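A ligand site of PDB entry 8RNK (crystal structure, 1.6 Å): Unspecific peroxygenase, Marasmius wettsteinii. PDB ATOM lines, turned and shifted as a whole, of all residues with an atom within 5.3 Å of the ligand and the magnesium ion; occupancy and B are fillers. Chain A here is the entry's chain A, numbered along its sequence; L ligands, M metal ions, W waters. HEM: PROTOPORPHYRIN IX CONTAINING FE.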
ATOM      1  N   PRO A  20      25.783   5.539  -0.173  1.00  0.00           N
ATOM      2  CA  PRO A  20      26.974   4.799  -0.583  1.00  0.00           C
ATOM      3  C   PRO A  20      26.987   3.333  -0.192  1.00  0.00           C
ATOM      4  O   PRO A  20      27.957   2.637  -0.470  1.00  0.00           O
ATOM      5  CB  PRO A  20      28.050   5.614   0.161  1.00  0.00           C
ATOM      6  CG  PRO A  20      27.375   5.919   1.484  1.00  0.00           C
ATOM      7  CD  PRO A  20      25.951   6.268   1.094  1.00  0.00           C
ATOM      8  N   CYS A  21      25.917   2.891   0.486  1.00  0.00           N
ATOM      9  CA  CYS A  21      25.823   1.530   1.003  1.00  0.00           C
ATOM     10  C   CYS A  21      24.934   0.671   0.096  1.00  0.00           C
ATOM     11  O   CYS A  21      23.724   0.871   0.073  1.00  0.00           O
ATOM     12  CB  CYS A  21      25.274   1.530   2.412  1.00  0.00           C
ATOM     13  SG  CYS A  21      25.053  -0.143   3.068  1.00  0.00           S
ATOM     14  N   PRO A  22      25.481  -0.372  -0.559  1.00  0.00           N
ATOM     15  CA  PRO A  22      24.644  -1.286  -1.335  1.00  0.00           C
ATOM     16  C   PRO A  22      23.677  -2.086  -0.456  1.00  0.00           C
ATOM     17  O   PRO A  22      22.613  -2.492  -0.928  1.00  0.00           O
ATOM     18  CB  PRO A  22      25.662  -2.197  -2.027  1.00  0.00           C
ATOM     19  CG  PRO A  22      26.844  -2.194  -1.098  1.00  0.00           C
ATOM     20  CD  PRO A  22      26.896  -0.757  -0.604  1.00  0.00           C
ATOM     21  N   GLY A  23      24.045  -2.328   0.802  1.00  0.00           N
ATOM     22  CA  GLY A  23      23.165  -3.090   1.683  1.00  0.00           C
ATOM     23  C   GLY A  23      21.837  -2.395   1.892  1.00  0.00           C
ATOM     24  O   GLY A  23      20.754  -2.973   1.710  1.00  0.00           O
ATOM     25  N   LEU A  24      21.905  -1.138   2.337  1.00  0.00           N
ATOM     26  CA  LEU A  24      20.710  -0.363   2.627  1.00  0.00           C
ATOM     27  C   LEU A  24      20.005   0.006   1.333  1.00  0.00           C
ATOM     28  O   LEU A  24      18.783   0.015   1.288  1.00  0.00           O
ATOM     29  CB  LEU A  24      21.068   0.875   3.439  1.00  0.00           C
ATOM     30  CG  LEU A  24      21.677   0.604   4.805  1.00  0.00           C
ATOM     31  CD1 LEU A  24      21.978   1.910   5.489  1.00  0.00           C
ATOM     32  CD2 LEU A  24      20.781  -0.278   5.664  1.00  0.00           C
ATOM     33  N   LEU A  27      17.927  -2.910   0.228  1.00  0.00           N
ATOM     34  CA  LEU A  27      16.740  -3.050   1.050  1.00  0.00           C
ATOM     35  C   LEU A  27      15.664  -2.043   0.614  1.00  0.00           C
ATOM     36  O   LEU A  27      14.482  -2.410   0.557  1.00  0.00           O
ATOM     37  CB  LEU A  27      17.087  -2.904   2.536  1.00  0.00           C
ATOM     38  CG  LEU A  27      17.910  -4.054   3.132  1.00  0.00           C
ATOM     39  CD1 LEU A  27      18.379  -3.688   4.522  1.00  0.00           C
ATOM     40  CD2 LEU A  27      17.139  -5.371   3.146  1.00  0.00           C
ATOM     41  N   ILE A  45      15.934   0.093  10.196  1.00  0.00           N
ATOM     42  CA  ILE A  45      17.091  -0.619   9.666  1.00  0.00           C
ATOM     43  C   ILE A  45      17.221  -2.014  10.284  1.00  0.00           C
ATOM     44  O   ILE A  45      17.523  -2.990   9.587  1.00  0.00           O
ATOM     45  CB  ILE A  45      18.372   0.225   9.871  1.00  0.00           C
ATOM     46  CG1 ILE A  45      18.339   1.488   9.023  1.00  0.00           C
ATOM     47  CG2 ILE A  45      19.583  -0.620   9.575  1.00  0.00           C
ATOM     48  CD1 ILE A  45      19.407   2.496   9.341  1.00  0.00           C
ATOM     49  N   TYR A  53      18.009 -10.003   5.115  1.00  0.00           N
ATOM     50  CA  TYR A  53      19.321 -10.613   5.053  1.00  0.00           C
ATOM     51  C   TYR A  53      19.613 -11.551   6.225  1.00  0.00           C
ATOM     52  O   TYR A  53      20.629 -12.245   6.196  1.00  0.00           O
ATOM     53  CB  TYR A  53      20.409  -9.528   5.080  1.00  0.00           C
ATOM     54  CG  TYR A  53      20.404  -8.482   3.997  1.00  0.00           C
ATOM     55  CD1 TYR A  53      20.151  -8.799   2.675  1.00  0.00           C
ATOM     56  CD2 TYR A  53      20.746  -7.165   4.274  1.00  0.00           C
ATOM     57  CE1 TYR A  53      20.194  -7.838   1.673  1.00  0.00           C
ATOM     58  CE2 TYR A  53      20.820  -6.198   3.273  1.00  0.00           C
ATOM     59  CZ  TYR A  53      20.534  -6.534   1.967  1.00  0.00           C
ATOM     60  OH  TYR A  53      20.588  -5.587   0.979  1.00  0.00           O
ATOM     61  N   VAL A  55      20.442 -10.368   9.041  1.00  0.00           N
ATOM     62  CA  VAL A  55      21.442  -9.680   9.846  1.00  0.00           C
ATOM     63  C   VAL A  55      20.800  -9.238  11.155  1.00  0.00           C
ATOM     64  O   VAL A  55      19.687  -8.707  11.152  1.00  0.00           O
ATOM     65  CB  VAL A  55      22.063  -8.497   9.071  1.00  0.00           C
ATOM     66  CG1 VAL A  55      22.988  -7.689   9.960  1.00  0.00           C
ATOM     67  CG2 VAL A  55      22.799  -8.971   7.842  1.00  0.00           C
ATOM     68  N   ILE A  59      24.873  -5.737  15.191  1.00  0.00           N
ATOM     69  CA  ILE A  59      25.668  -4.926  14.276  1.00  0.00           C
ATOM     70  C   ILE A  59      24.819  -3.761  13.770  1.00  0.00           C
ATOM     71  O   ILE A  59      25.357  -2.683  13.552  1.00  0.00           O
ATOM     72  CB  ILE A  59      26.283  -5.759  13.126  1.00  0.00           C
ATOM     73  CG1 ILE A  59      27.238  -4.923  12.272  1.00  0.00           C
ATOM     74  CG2 ILE A  59      25.214  -6.415  12.293  1.00  0.00           C
ATOM     75  CD1 ILE A  59      28.139  -5.732  11.366  1.00  0.00           C
ATOM     76  N   LEU A  60      23.521  -3.948  13.571  1.00  0.00           N
ATOM     77  CA  LEU A  60      22.716  -2.909  12.941  1.00  0.00           C
ATOM     78  C   LEU A  60      22.440  -1.757  13.889  1.00  0.00           C
ATOM     79  O   LEU A  60      22.328  -0.617  13.447  1.00  0.00           O
ATOM     80  CB  LEU A  60      21.424  -3.501  12.353  1.00  0.00           C
ATOM     81  CG  LEU A  60      21.671  -4.498  11.237  1.00  0.00           C
ATOM     82  CD1 LEU A  60      20.366  -5.098  10.757  1.00  0.00           C
ATOM     83  CD2 LEU A  60      22.415  -3.848  10.064  1.00  0.00           C
ATOM     84  N   ALA A  63      26.122   0.098  14.074  1.00  0.00           N
ATOM     85  CA  ALA A  63      26.364   0.852  12.850  1.00  0.00           C
ATOM     86  C   ALA A  63      25.264   1.889  12.609  1.00  0.00           C
ATOM     87  O   ALA A  63      25.538   3.033  12.214  1.00  0.00           O
ATOM     88  CB  ALA A  63      26.479  -0.117  11.697  1.00  0.00           C
ATOM     89  N   GLY A  64      24.005   1.507  12.842  1.00  0.00           N
ATOM     90  CA  GLY A  64      22.882   2.382  12.610  1.00  0.00           C
ATOM     91  C   GLY A  64      22.981   3.696  13.379  1.00  0.00           C
ATOM     92  O   GLY A  64      22.699   4.760  12.834  1.00  0.00           O
ATOM     93  N   GLY A  67      25.440   5.884  11.907  1.00  0.00           N
ATOM     94  CA  GLY A  67      24.889   6.471  10.685  1.00  0.00           C
ATOM     95  C   GLY A  67      23.935   7.621  10.954  1.00  0.00           C
ATOM     96  O   GLY A  67      23.835   8.558  10.186  1.00  0.00           O
ATOM     97  N   LEU A  82      24.268   9.353   4.407  1.00  0.00           N
ATOM     98  CA  LEU A  82      25.367   8.477   4.801  1.00  0.00           C
ATOM     99  C   LEU A  82      26.635   8.701   3.981  1.00  0.00           C
ATOM    100  O   LEU A  82      27.693   8.166   4.329  1.00  0.00           O
ATOM    101  CB  LEU A  82      24.891   7.030   4.656  1.00  0.00           C
ATOM    102  CG  LEU A  82      23.826   6.581   5.639  1.00  0.00           C
ATOM    103  CD1 LEU A  82      23.336   5.181   5.299  1.00  0.00           C
ATOM    104  CD2 LEU A  82      24.350   6.627   7.047  1.00  0.00           C
ATOM    105  N   ILE A  88      30.990   7.286   8.626  1.00  0.00           N
ATOM    106  CA  ILE A  88      31.274   5.935   8.171  1.00  0.00           C
ATOM    107  C   ILE A  88      31.978   5.962   6.807  1.00  0.00           C
ATOM    108  O   ILE A  88      32.960   5.254   6.604  1.00  0.00           O
ATOM    109  CB  ILE A  88      29.993   5.083   8.132  1.00  0.00           C
ATOM    110  CG1 ILE A  88      29.391   4.928   9.530  1.00  0.00           C
ATOM    111  CG2 ILE A  88      30.267   3.724   7.526  1.00  0.00           C
ATOM    112  CD1 ILE A  88      27.980   4.398   9.494  1.00  0.00           C
ATOM    113  N   GLU A  89      31.494   6.801   5.893  1.00  0.00           N
ATOM    114  CA  GLU A  89      32.017   6.825   4.532  1.00  0.00           C
ATOM    115  C   GLU A  89      33.524   7.098   4.564  1.00  0.00           C
ATOM    116  O   GLU A  89      33.997   7.948   5.324  1.00  0.00           O
ATOM    117  CB  GLU A  89      31.263   7.831   3.673  1.00  0.00           C
ATOM    118  CG  GLU A  89      31.533   7.651   2.190  1.00  0.00           C
ATOM    119  CD  GLU A  89      32.869   8.202   1.727  1.00  0.00           C
ATOM    120  OE1 GLU A  89      33.202   9.306   2.181  1.00  0.00           O
ATOM    121  OE2 GLU A  89      33.494   7.563   0.882  1.00  0.00           O
ATOM    122  N   HIS A  90      34.245   6.343   3.757  1.00  0.00           N
ATOM    123  CA  HIS A  90      35.702   6.325   3.785  1.00  0.00           C
ATOM    124  C   HIS A  90      36.266   6.230   2.370  1.00  0.00           C
ATOM    125  O   HIS A  90      35.625   5.766   1.434  1.00  0.00           O
ATOM    126  CB  HIS A  90      36.213   5.143   4.627  1.00  0.00           C
ATOM    127  CG  HIS A  90      35.589   3.853   4.233  1.00  0.00           C
ATOM    128  ND1 HIS A  90      35.978   3.194   3.096  1.00  0.00           N
ATOM    129  CD2 HIS A  90      34.560   3.129   4.739  1.00  0.00           C
ATOM    130  CE1 HIS A  90      35.206   2.128   2.920  1.00  0.00           C
ATOM    131  NE2 HIS A  90      34.347   2.065   3.906  1.00  0.00           N
ATOM    132  N   ASP A  91      37.562   6.524   2.276  1.00  0.00           N
ATOM    133  CA  ASP A  91      38.328   6.289   1.067  1.00  0.00           C
ATOM    134  C   ASP A  91      38.543   4.793   0.860  1.00  0.00           C
ATOM    135  O   ASP A  91      38.323   4.002   1.778  1.00  0.00           O
ATOM    136  CB  ASP A  91      39.666   7.006   1.180  1.00  0.00           C
ATOM    137  CG  ASP A  91      39.516   8.505   1.296  1.00  0.00           C
ATOM    138  OD1 ASP A  91      38.520   9.047   0.766  1.00  0.00           O
ATOM    139  OD2 ASP A  91      40.412   9.143   1.907  1.00  0.00           O
ATOM    140  N   SER A  93      36.917   2.712  -1.010  1.00  0.00           N
ATOM    141  CA  SER A  93      35.708   1.917  -1.151  1.00  0.00           C
ATOM    142  C   SER A  93      35.869   0.903  -2.293  1.00  0.00           C
ATOM    143  O   SER A  93      36.701   1.077  -3.164  1.00  0.00           O
ATOM    144  CB  SER A  93      34.526   2.818  -1.404  1.00  0.00           C
ATOM    145  OG  SER A  93      34.233   3.605  -0.255  1.00  0.00           O
ATOM    146  N   LEU A  94      34.978  -0.099  -2.330  1.00  0.00           N
ATOM    147  CA  LEU A  94      35.023  -1.173  -3.305  1.00  0.00           C
ATOM    148  C   LEU A  94      34.362  -0.757  -4.611  1.00  0.00           C
ATOM    149  O   LEU A  94      34.642  -1.380  -5.638  1.00  0.00           O
ATOM    150  CB  LEU A  94      34.266  -2.369  -2.735  1.00  0.00           C
ATOM    151  CG  LEU A  94      34.842  -2.981  -1.462  1.00  0.00           C
ATOM    152  CD1 LEU A  94      33.813  -3.881  -0.778  1.00  0.00           C
ATOM    153  CD2 LEU A  94      36.124  -3.726  -1.745  1.00  0.00           C
ATOM    154  N   SER A  95      33.448   0.215  -4.555  1.00  0.00           N
ATOM    155  CA  SER A  95      32.587   0.504  -5.706  1.00  0.00           C
ATOM    156  C   SER A  95      32.321   1.997  -5.887  1.00  0.00           C
ATOM    157  O   SER A  95      31.566   2.360  -6.782  1.00  0.00           O
ATOM    158  CB  SER A  95      31.273  -0.278  -5.599  1.00  0.00           C
ATOM    159  OG  SER A  95      30.464   0.176  -4.524  1.00  0.00           O
ATOM    160  N   ARG A  96      32.910   2.846  -5.039  1.00  0.00           N
ATOM    161  CA  ARG A  96      32.753   4.288  -5.097  1.00  0.00           C
ATOM    162  C   ARG A  96      34.144   4.923  -5.175  1.00  0.00           C
ATOM    163  O   ARG A  96      35.127   4.293  -4.770  1.00  0.00           O
ATOM    164  CB  ARG A  96      32.038   4.858  -3.869  1.00  0.00           C
ATOM    165  CG  ARG A  96      30.504   4.864  -3.920  1.00  0.00           C
ATOM    166  CD  ARG A  96      29.852   3.536  -4.135  1.00  0.00           C
ATOM    167  NE  ARG A  96      28.413   3.639  -3.985  1.00  0.00           N
ATOM    168  CZ  ARG A  96      27.516   2.666  -4.190  1.00  0.00           C
ATOM    169  NH1 ARG A  96      27.890   1.447  -4.525  1.00  0.00           N
ATOM    170  NH2 ARG A  96      26.231   2.944  -4.082  1.00  0.00           N
ATOM    171  N   GLU A  97      34.190   6.179  -5.640  1.00  0.00           N
ATOM    172  CA  GLU A  97      35.444   6.922  -5.697  1.00  0.00           C
ATOM    173  C   GLU A  97      35.651   7.627  -4.360  1.00  0.00           C
ATOM    174  O   GLU A  97      34.696   7.867  -3.630  1.00  0.00           O
ATOM    175  CB  GLU A  97      35.401   7.949  -6.842  1.00  0.00           C
ATOM    176  CG  GLU A  97      35.175   7.320  -8.203  1.00  0.00           C
ATOM    177  CD  GLU A  97      35.018   8.331  -9.326  1.00  0.00           C
ATOM    178  OE1 GLU A  97      34.353   9.362  -9.115  1.00  0.00           O
ATOM    179  OE2 GLU A  97      35.574   8.070 -10.425  1.00  0.00           O
ATOM    180  N   ASN A 104      31.764   9.966  -4.197  1.00  0.00           N
ATOM    181  CA  ASN A 104      31.819   9.010  -3.095  1.00  0.00           C
ATOM    182  C   ASN A 104      30.465   8.383  -2.814  1.00  0.00           C
ATOM    183  O   ASN A 104      30.334   7.712  -1.796  1.00  0.00           O
ATOM    184  CB  ASN A 104      32.363   9.650  -1.816  1.00  0.00           C
ATOM    185  CG  ASN A 104      31.387  10.561  -1.114  1.00  0.00           C
ATOM    186  OD1 ASN A 104      30.441  11.041  -1.723  1.00  0.00           O
ATOM    187  ND2 ASN A 104      31.577  10.769   0.180  1.00  0.00           N
ATOM    188  N   GLU A 161      32.708  -4.348   5.791  1.00  0.00           N
ATOM    189  CA  GLU A 161      31.909  -4.253   4.572  1.00  0.00           C
ATOM    190  C   GLU A 161      32.178  -5.446   3.655  1.00  0.00           C
ATOM    191  O   GLU A 161      31.257  -6.006   3.065  1.00  0.00           O
ATOM    192  CB  GLU A 161      32.164  -2.899   3.923  1.00  0.00           C
ATOM    193  CG  GLU A 161      31.531  -1.784   4.744  1.00  0.00           C
ATOM    194  CD  GLU A 161      32.083  -0.373   4.589  1.00  0.00           C
ATOM    195  OE1 GLU A 161      33.029  -0.190   3.862  1.00  0.00           O
ATOM    196  OE2 GLU A 161      31.469   0.512   5.213  1.00  0.00           O
ATOM    197  N   SER A 162      33.448  -5.845   3.526  1.00  0.00           N
ATOM    198  CA  SER A 162      33.776  -7.050   2.771  1.00  0.00           C
ATOM    199  C   SER A 162      33.137  -8.283   3.425  1.00  0.00           C
ATOM    200  O   SER A 162      32.564  -9.128   2.720  1.00  0.00           O
ATOM    201  CB  SER A 162      35.269  -7.239   2.619  1.00  0.00           C
ATOM    202  OG  SER A 162      35.836  -6.183   1.842  1.00  0.00           O
ATOM    203  N   PHE A 164      30.389  -8.312   5.075  1.00  0.00           N
ATOM    204  CA  PHE A 164      28.976  -8.223   4.760  1.00  0.00           C
ATOM    205  C   PHE A 164      28.689  -8.839   3.397  1.00  0.00           C
ATOM    206  O   PHE A 164      27.747  -9.635   3.264  1.00  0.00           O
ATOM    207  CB  PHE A 164      28.462  -6.778   4.818  1.00  0.00           C
ATOM    208  CG  PHE A 164      27.837  -6.365   6.113  1.00  0.00           C
ATOM    209  CD1 PHE A 164      26.968  -7.220   6.774  1.00  0.00           C
ATOM    210  CD2 PHE A 164      27.961  -5.051   6.560  1.00  0.00           C
ATOM    211  CE1 PHE A 164      26.334  -6.813   7.943  1.00  0.00           C
ATOM    212  CE2 PHE A 164      27.319  -4.656   7.730  1.00  0.00           C
ATOM    213  CZ  PHE A 164      26.508  -5.528   8.406  1.00  0.00           C
ATOM    214  N   TYR A 165      29.440  -8.453   2.349  1.00  0.00           N
ATOM    215  CA  TYR A 165      29.079  -8.971   1.033  1.00  0.00           C
ATOM    216  C   TYR A 165      29.344 -10.472   0.943  1.00  0.00           C
ATOM    217  O   TYR A 165      28.545 -11.183   0.322  1.00  0.00           O
ATOM    218  CB  TYR A 165      29.660  -8.147  -0.142  1.00  0.00           C
ATOM    219  CG  TYR A 165      31.096  -8.379  -0.528  1.00  0.00           C
ATOM    220  CD1 TYR A 165      31.498  -9.551  -1.147  1.00  0.00           C
ATOM    221  CD2 TYR A 165      32.047  -7.407  -0.318  1.00  0.00           C
ATOM    222  CE1 TYR A 165      32.798  -9.759  -1.556  1.00  0.00           C
ATOM    223  CE2 TYR A 165      33.375  -7.593  -0.699  1.00  0.00           C
ATOM    224  CZ  TYR A 165      33.750  -8.775  -1.327  1.00  0.00           C
ATOM    225  OH  TYR A 165      35.082  -8.931  -1.658  1.00  0.00           O
ATOM    226  N   VAL A 168      26.153 -11.969   3.473  1.00  0.00           N
ATOM    227  CA  VAL A 168      24.755 -11.729   3.151  1.00  0.00           C
ATOM    228  C   VAL A 168      24.401 -12.310   1.784  1.00  0.00           C
ATOM    229  O   VAL A 168      23.256 -12.751   1.572  1.00  0.00           O
ATOM    230  CB  VAL A 168      24.454 -10.218   3.267  1.00  0.00           C
ATOM    231  CG1 VAL A 168      23.141  -9.840   2.660  1.00  0.00           C
ATOM    232  CG2 VAL A 168      24.548  -9.729   4.703  1.00  0.00           C
ATOM    233  N   PHE A 187      24.331  -7.595  -6.549  1.00  0.00           N
ATOM    234  CA  PHE A 187      24.183  -6.793  -5.354  1.00  0.00           C
ATOM    235  C   PHE A 187      24.794  -5.410  -5.551  1.00  0.00           C
ATOM    236  O   PHE A 187      24.145  -4.407  -5.292  1.00  0.00           O
ATOM    237  CB  PHE A 187      24.763  -7.594  -4.183  1.00  0.00           C
ATOM    238  CG  PHE A 187      24.777  -6.901  -2.857  1.00  0.00           C
ATOM    239  CD1 PHE A 187      23.603  -6.671  -2.166  1.00  0.00           C
ATOM    240  CD2 PHE A 187      25.975  -6.498  -2.287  1.00  0.00           C
ATOM    241  CE1 PHE A 187      23.612  -6.032  -0.929  1.00  0.00           C
ATOM    242  CE2 PHE A 187      25.977  -5.878  -1.042  1.00  0.00           C
ATOM    243  CZ  PHE A 187      24.796  -5.639  -0.372  1.00  0.00           C
ATOM    244  N   PHE A 188      26.041  -5.351  -6.050  1.00  0.00           N
ATOM    245  CA  PHE A 188      26.710  -4.069  -6.214  1.00  0.00           C
ATOM    246  C   PHE A 188      26.202  -3.308  -7.451  1.00  0.00           C
ATOM    247  O   PHE A 188      25.923  -2.116  -7.386  1.00  0.00           O
ATOM    248  CB  PHE A 188      28.226  -4.297  -6.358  1.00  0.00           C
ATOM    249  CG  PHE A 188      28.988  -4.405  -5.054  1.00  0.00           C
ATOM    250  CD1 PHE A 188      29.423  -3.265  -4.387  1.00  0.00           C
ATOM    251  CD2 PHE A 188      29.263  -5.630  -4.481  1.00  0.00           C
ATOM    252  CE1 PHE A 188      30.136  -3.368  -3.200  1.00  0.00           C
ATOM    253  CE2 PHE A 188      29.972  -5.729  -3.285  1.00  0.00           C
ATOM    254  CZ  PHE A 188      30.423  -4.596  -2.656  1.00  0.00           C
HETATM  255  CHA HEM L   1      29.272   0.581   2.687  1.00  0.00           C
HETATM  256  CHB HEM L   1      26.488   2.396   6.197  1.00  0.00           C
HETATM  257  CHC HEM L   1      24.360  -1.906   6.705  1.00  0.00           C
HETATM  258  CHD HEM L   1      27.019  -3.694   3.076  1.00  0.00           C
HETATM  259  C1A HEM L   1      28.650   1.448   3.541  1.00  0.00           C
HETATM  260  C2A HEM L   1      28.906   2.842   3.633  1.00  0.00           C
HETATM  261  C3A HEM L   1      28.155   3.361   4.606  1.00  0.00           C
HETATM  262  C4A HEM L   1      27.379   2.283   5.143  1.00  0.00           C
HETATM  263  CMA HEM L   1      28.077   4.808   5.012  1.00  0.00           C
HETATM  264  CAA HEM L   1      29.879   3.587   2.760  1.00  0.00           C
HETATM  265  CBA HEM L   1      31.304   3.316   3.261  1.00  0.00           C
HETATM  266  CGA HEM L   1      32.275   3.509   2.108  1.00  0.00           C
HETATM  267  O1A HEM L   1      32.928   4.606   1.992  1.00  0.00           O
HETATM  268  O2A HEM L   1      32.413   2.603   1.235  1.00  0.00           O
HETATM  269  C1B HEM L   1      25.699   1.351   6.674  1.00  0.00           C
HETATM  270  C2B HEM L   1      24.811   1.501   7.810  1.00  0.00           C
HETATM  271  C3B HEM L   1      24.191   0.273   7.936  1.00  0.00           C
HETATM  272  C4B HEM L   1      24.747  -0.605   6.902  1.00  0.00           C
HETATM  273  CMB HEM L   1      24.538   2.750   8.585  1.00  0.00           C
HETATM  274  CAB HEM L   1      23.265  -0.333   8.913  1.00  0.00           C
HETATM  275  CBB HEM L   1      23.504  -0.135  10.176  1.00  0.00           C
HETATM  276  C1C HEM L   1      24.808  -2.757   5.724  1.00  0.00           C
HETATM  277  C2C HEM L   1      24.293  -4.035   5.420  1.00  0.00           C
HETATM  278  C3C HEM L   1      25.067  -4.542   4.403  1.00  0.00           C
HETATM  279  C4C HEM L   1      26.067  -3.572   4.042  1.00  0.00           C
HETATM  280  CMC HEM L   1      23.140  -4.734   6.121  1.00  0.00           C
HETATM  281  CAC HEM L   1      24.821  -5.899   3.837  1.00  0.00           C
HETATM  282  CBC HEM L   1      25.481  -6.464   2.851  1.00  0.00           C
HETATM  283  C1D HEM L   1      27.918  -2.645   2.695  1.00  0.00           C
HETATM  284  C2D HEM L   1      29.006  -2.834   1.699  1.00  0.00           C
HETATM  285  C3D HEM L   1      29.603  -1.619   1.618  1.00  0.00           C
HETATM  286  C4D HEM L   1      28.887  -0.747   2.543  1.00  0.00           C
HETATM  287  CMD HEM L   1      29.318  -4.117   0.975  1.00  0.00           C
HETATM  288  CAD HEM L   1      30.797  -1.298   0.782  1.00  0.00           C
HETATM  289  CBD HEM L   1      30.550  -0.440  -0.437  1.00  0.00           C
HETATM  290  CGD HEM L   1      31.828  -0.092  -1.129  1.00  0.00           C
HETATM  291  O1D HEM L   1      31.794   0.374  -2.294  1.00  0.00           O
HETATM  292  O2D HEM L   1      32.920  -0.226  -0.529  1.00  0.00           O
HETATM  293  NA  HEM L   1      27.739   1.122   4.533  1.00  0.00           N
HETATM  294  NB  HEM L   1      25.680   0.094   6.218  1.00  0.00           N
HETATM  295  NC  HEM L   1      25.810  -2.490   4.848  1.00  0.00           N
HETATM  296  ND  HEM L   1      27.890  -1.396   3.228  1.00  0.00           N
HETATM  297 FE   HEM L   1      26.727  -0.623   4.559  1.00  0.00          FE
HETATM  298 MG    MG M   1      33.819   5.611   0.331  1.00  0.00          MG
HETATM  299  O   HOH W   1      34.818   6.250  -1.383  1.00  0.00           O
HETATM  300  O   HOH W   2      31.932   5.645  -0.611  1.00  0.00           O
HETATM  301  O   HOH W   3      34.414  -0.746   1.595  1.00  0.00           O
HETATM  302  O   HOH W   4      30.601   3.247  -0.913  1.00  0.00           O
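Water W3 bridges O2D of the ligand (2.6 Å) and OE1 of Glu 161 (2.7 Å). Water W4 lies within hydrogen-bond range of the backbone carbonyl oxygen of Pro 20 and an oxygen (O2A) of the ligand.
The side-chain hydroxyl of Ser 95 lies within hydrogen-bond range of the guanidinium group of Arg 96 (2.9 Å). The side-chain amide nitrogen (ND2) of Asn 104 is in hydrogen-bond range of the side-chain carboxylate (OE1) of Glu 89. SG of Cys 21 sits close to N of Leu 24 (3.4 Å). The side-chain hydroxyl (OH) of Tyr 53 is in hydrogen-bond range of the backbone carbonyl oxygen (O) of Gly 23, at 2.7 Å. A ring nitrogen (NE2) of His 90 is in hydrogen-bond range of the side-chain carboxylate of Glu 161, 2.6 Å away. SG of Cys 21 sits close to N of Gly 23 (3.3 Å).
Pro 20 touches the ligand. Pro 22 touches the ligand. Gly 23 touches the ligand (CA to C3C, 3.6 Å). Leu 24 touches the ligand. Ile 45 touches the ligand. Tyr 53 touches the ligand (CD2 to CMC, 3.9 Å). Leu 60 touches the ligand. Ala 63 touches the ligand. N of Gly 64 touches CBB of the ligand, at 3.2 Å. O of Leu 82 touches CMA of the ligand, 3.4 Å away. CG2 of Ile 88 touches CMA of the ligand (3.5 Å). Arg 96 touches the ligand (N to O1D, 3.9 Å). Glu 161 touches the ligand. CD2 of Phe 164 touches C4C of the ligand, at 3.5 Å. CG2 of Val 168 touches CBC of the ligand (3.9 Å). CZ of Phe 187 touches CBC of the ligand (3.4 Å). Phe 188 touches the ligand (CZ to CMD, 3.8 Å). Hydrophobic or aromatic side chains that line the ligand: Pro 20, Pro 22, Leu 24, Ile 45, Tyr 53, Leu 60, Ala 63, Leu 82, Ile 88, His 90, Leu 94, Phe 164, Val 168, Phe 187 and Phe 188. Of the 32 residues printed, 23 come within 4 Å of the ligand. The nearest printed residue that does not touch the ligand is Tyr 165 (4.2 Å).
Three residues have an atom within 4 Å of the magnesium ion: Glu 89, His 90 and Ser 93.
The magnesium ion is bound by the side-chain carboxylate (OE2) of Glu 89 (2.1 Å), water W1 (2.1 Å), water W2 (2.1 Å), the backbone carbonyl oxygen (O) of His 90 (2.1 Å), the side-chain hydroxyl (OG) of Ser 93 (2.1 Å) and an oxygen (O1A) of the ligand (2.1 Å).
An oxygen (O1A) of the ligand sits close to the backbone NH (N) of His 90, at 2.8 Å. An oxygen (O2A) of the ligand lies close to a ring nitrogen (NE2) of His 90 (3.3 Å). An oxygen (O2D) of the ligand lies within hydrogen-bond range of the backbone NH (N) of Leu 94 (2.7 Å). The backbone NH of Ser 95 is in hydrogen-bond range of an oxygen (O1D) of the ligand (2.8 Å). An iron atom (FE) of the ligand is bound by the side-chain sulfur of Cys 21 (2.3 Å). An oxygen (O1D) of the ligand is in hydrogen-bond range of the side-chain hydroxyl (OG) of Ser 95 (2.6 Å).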
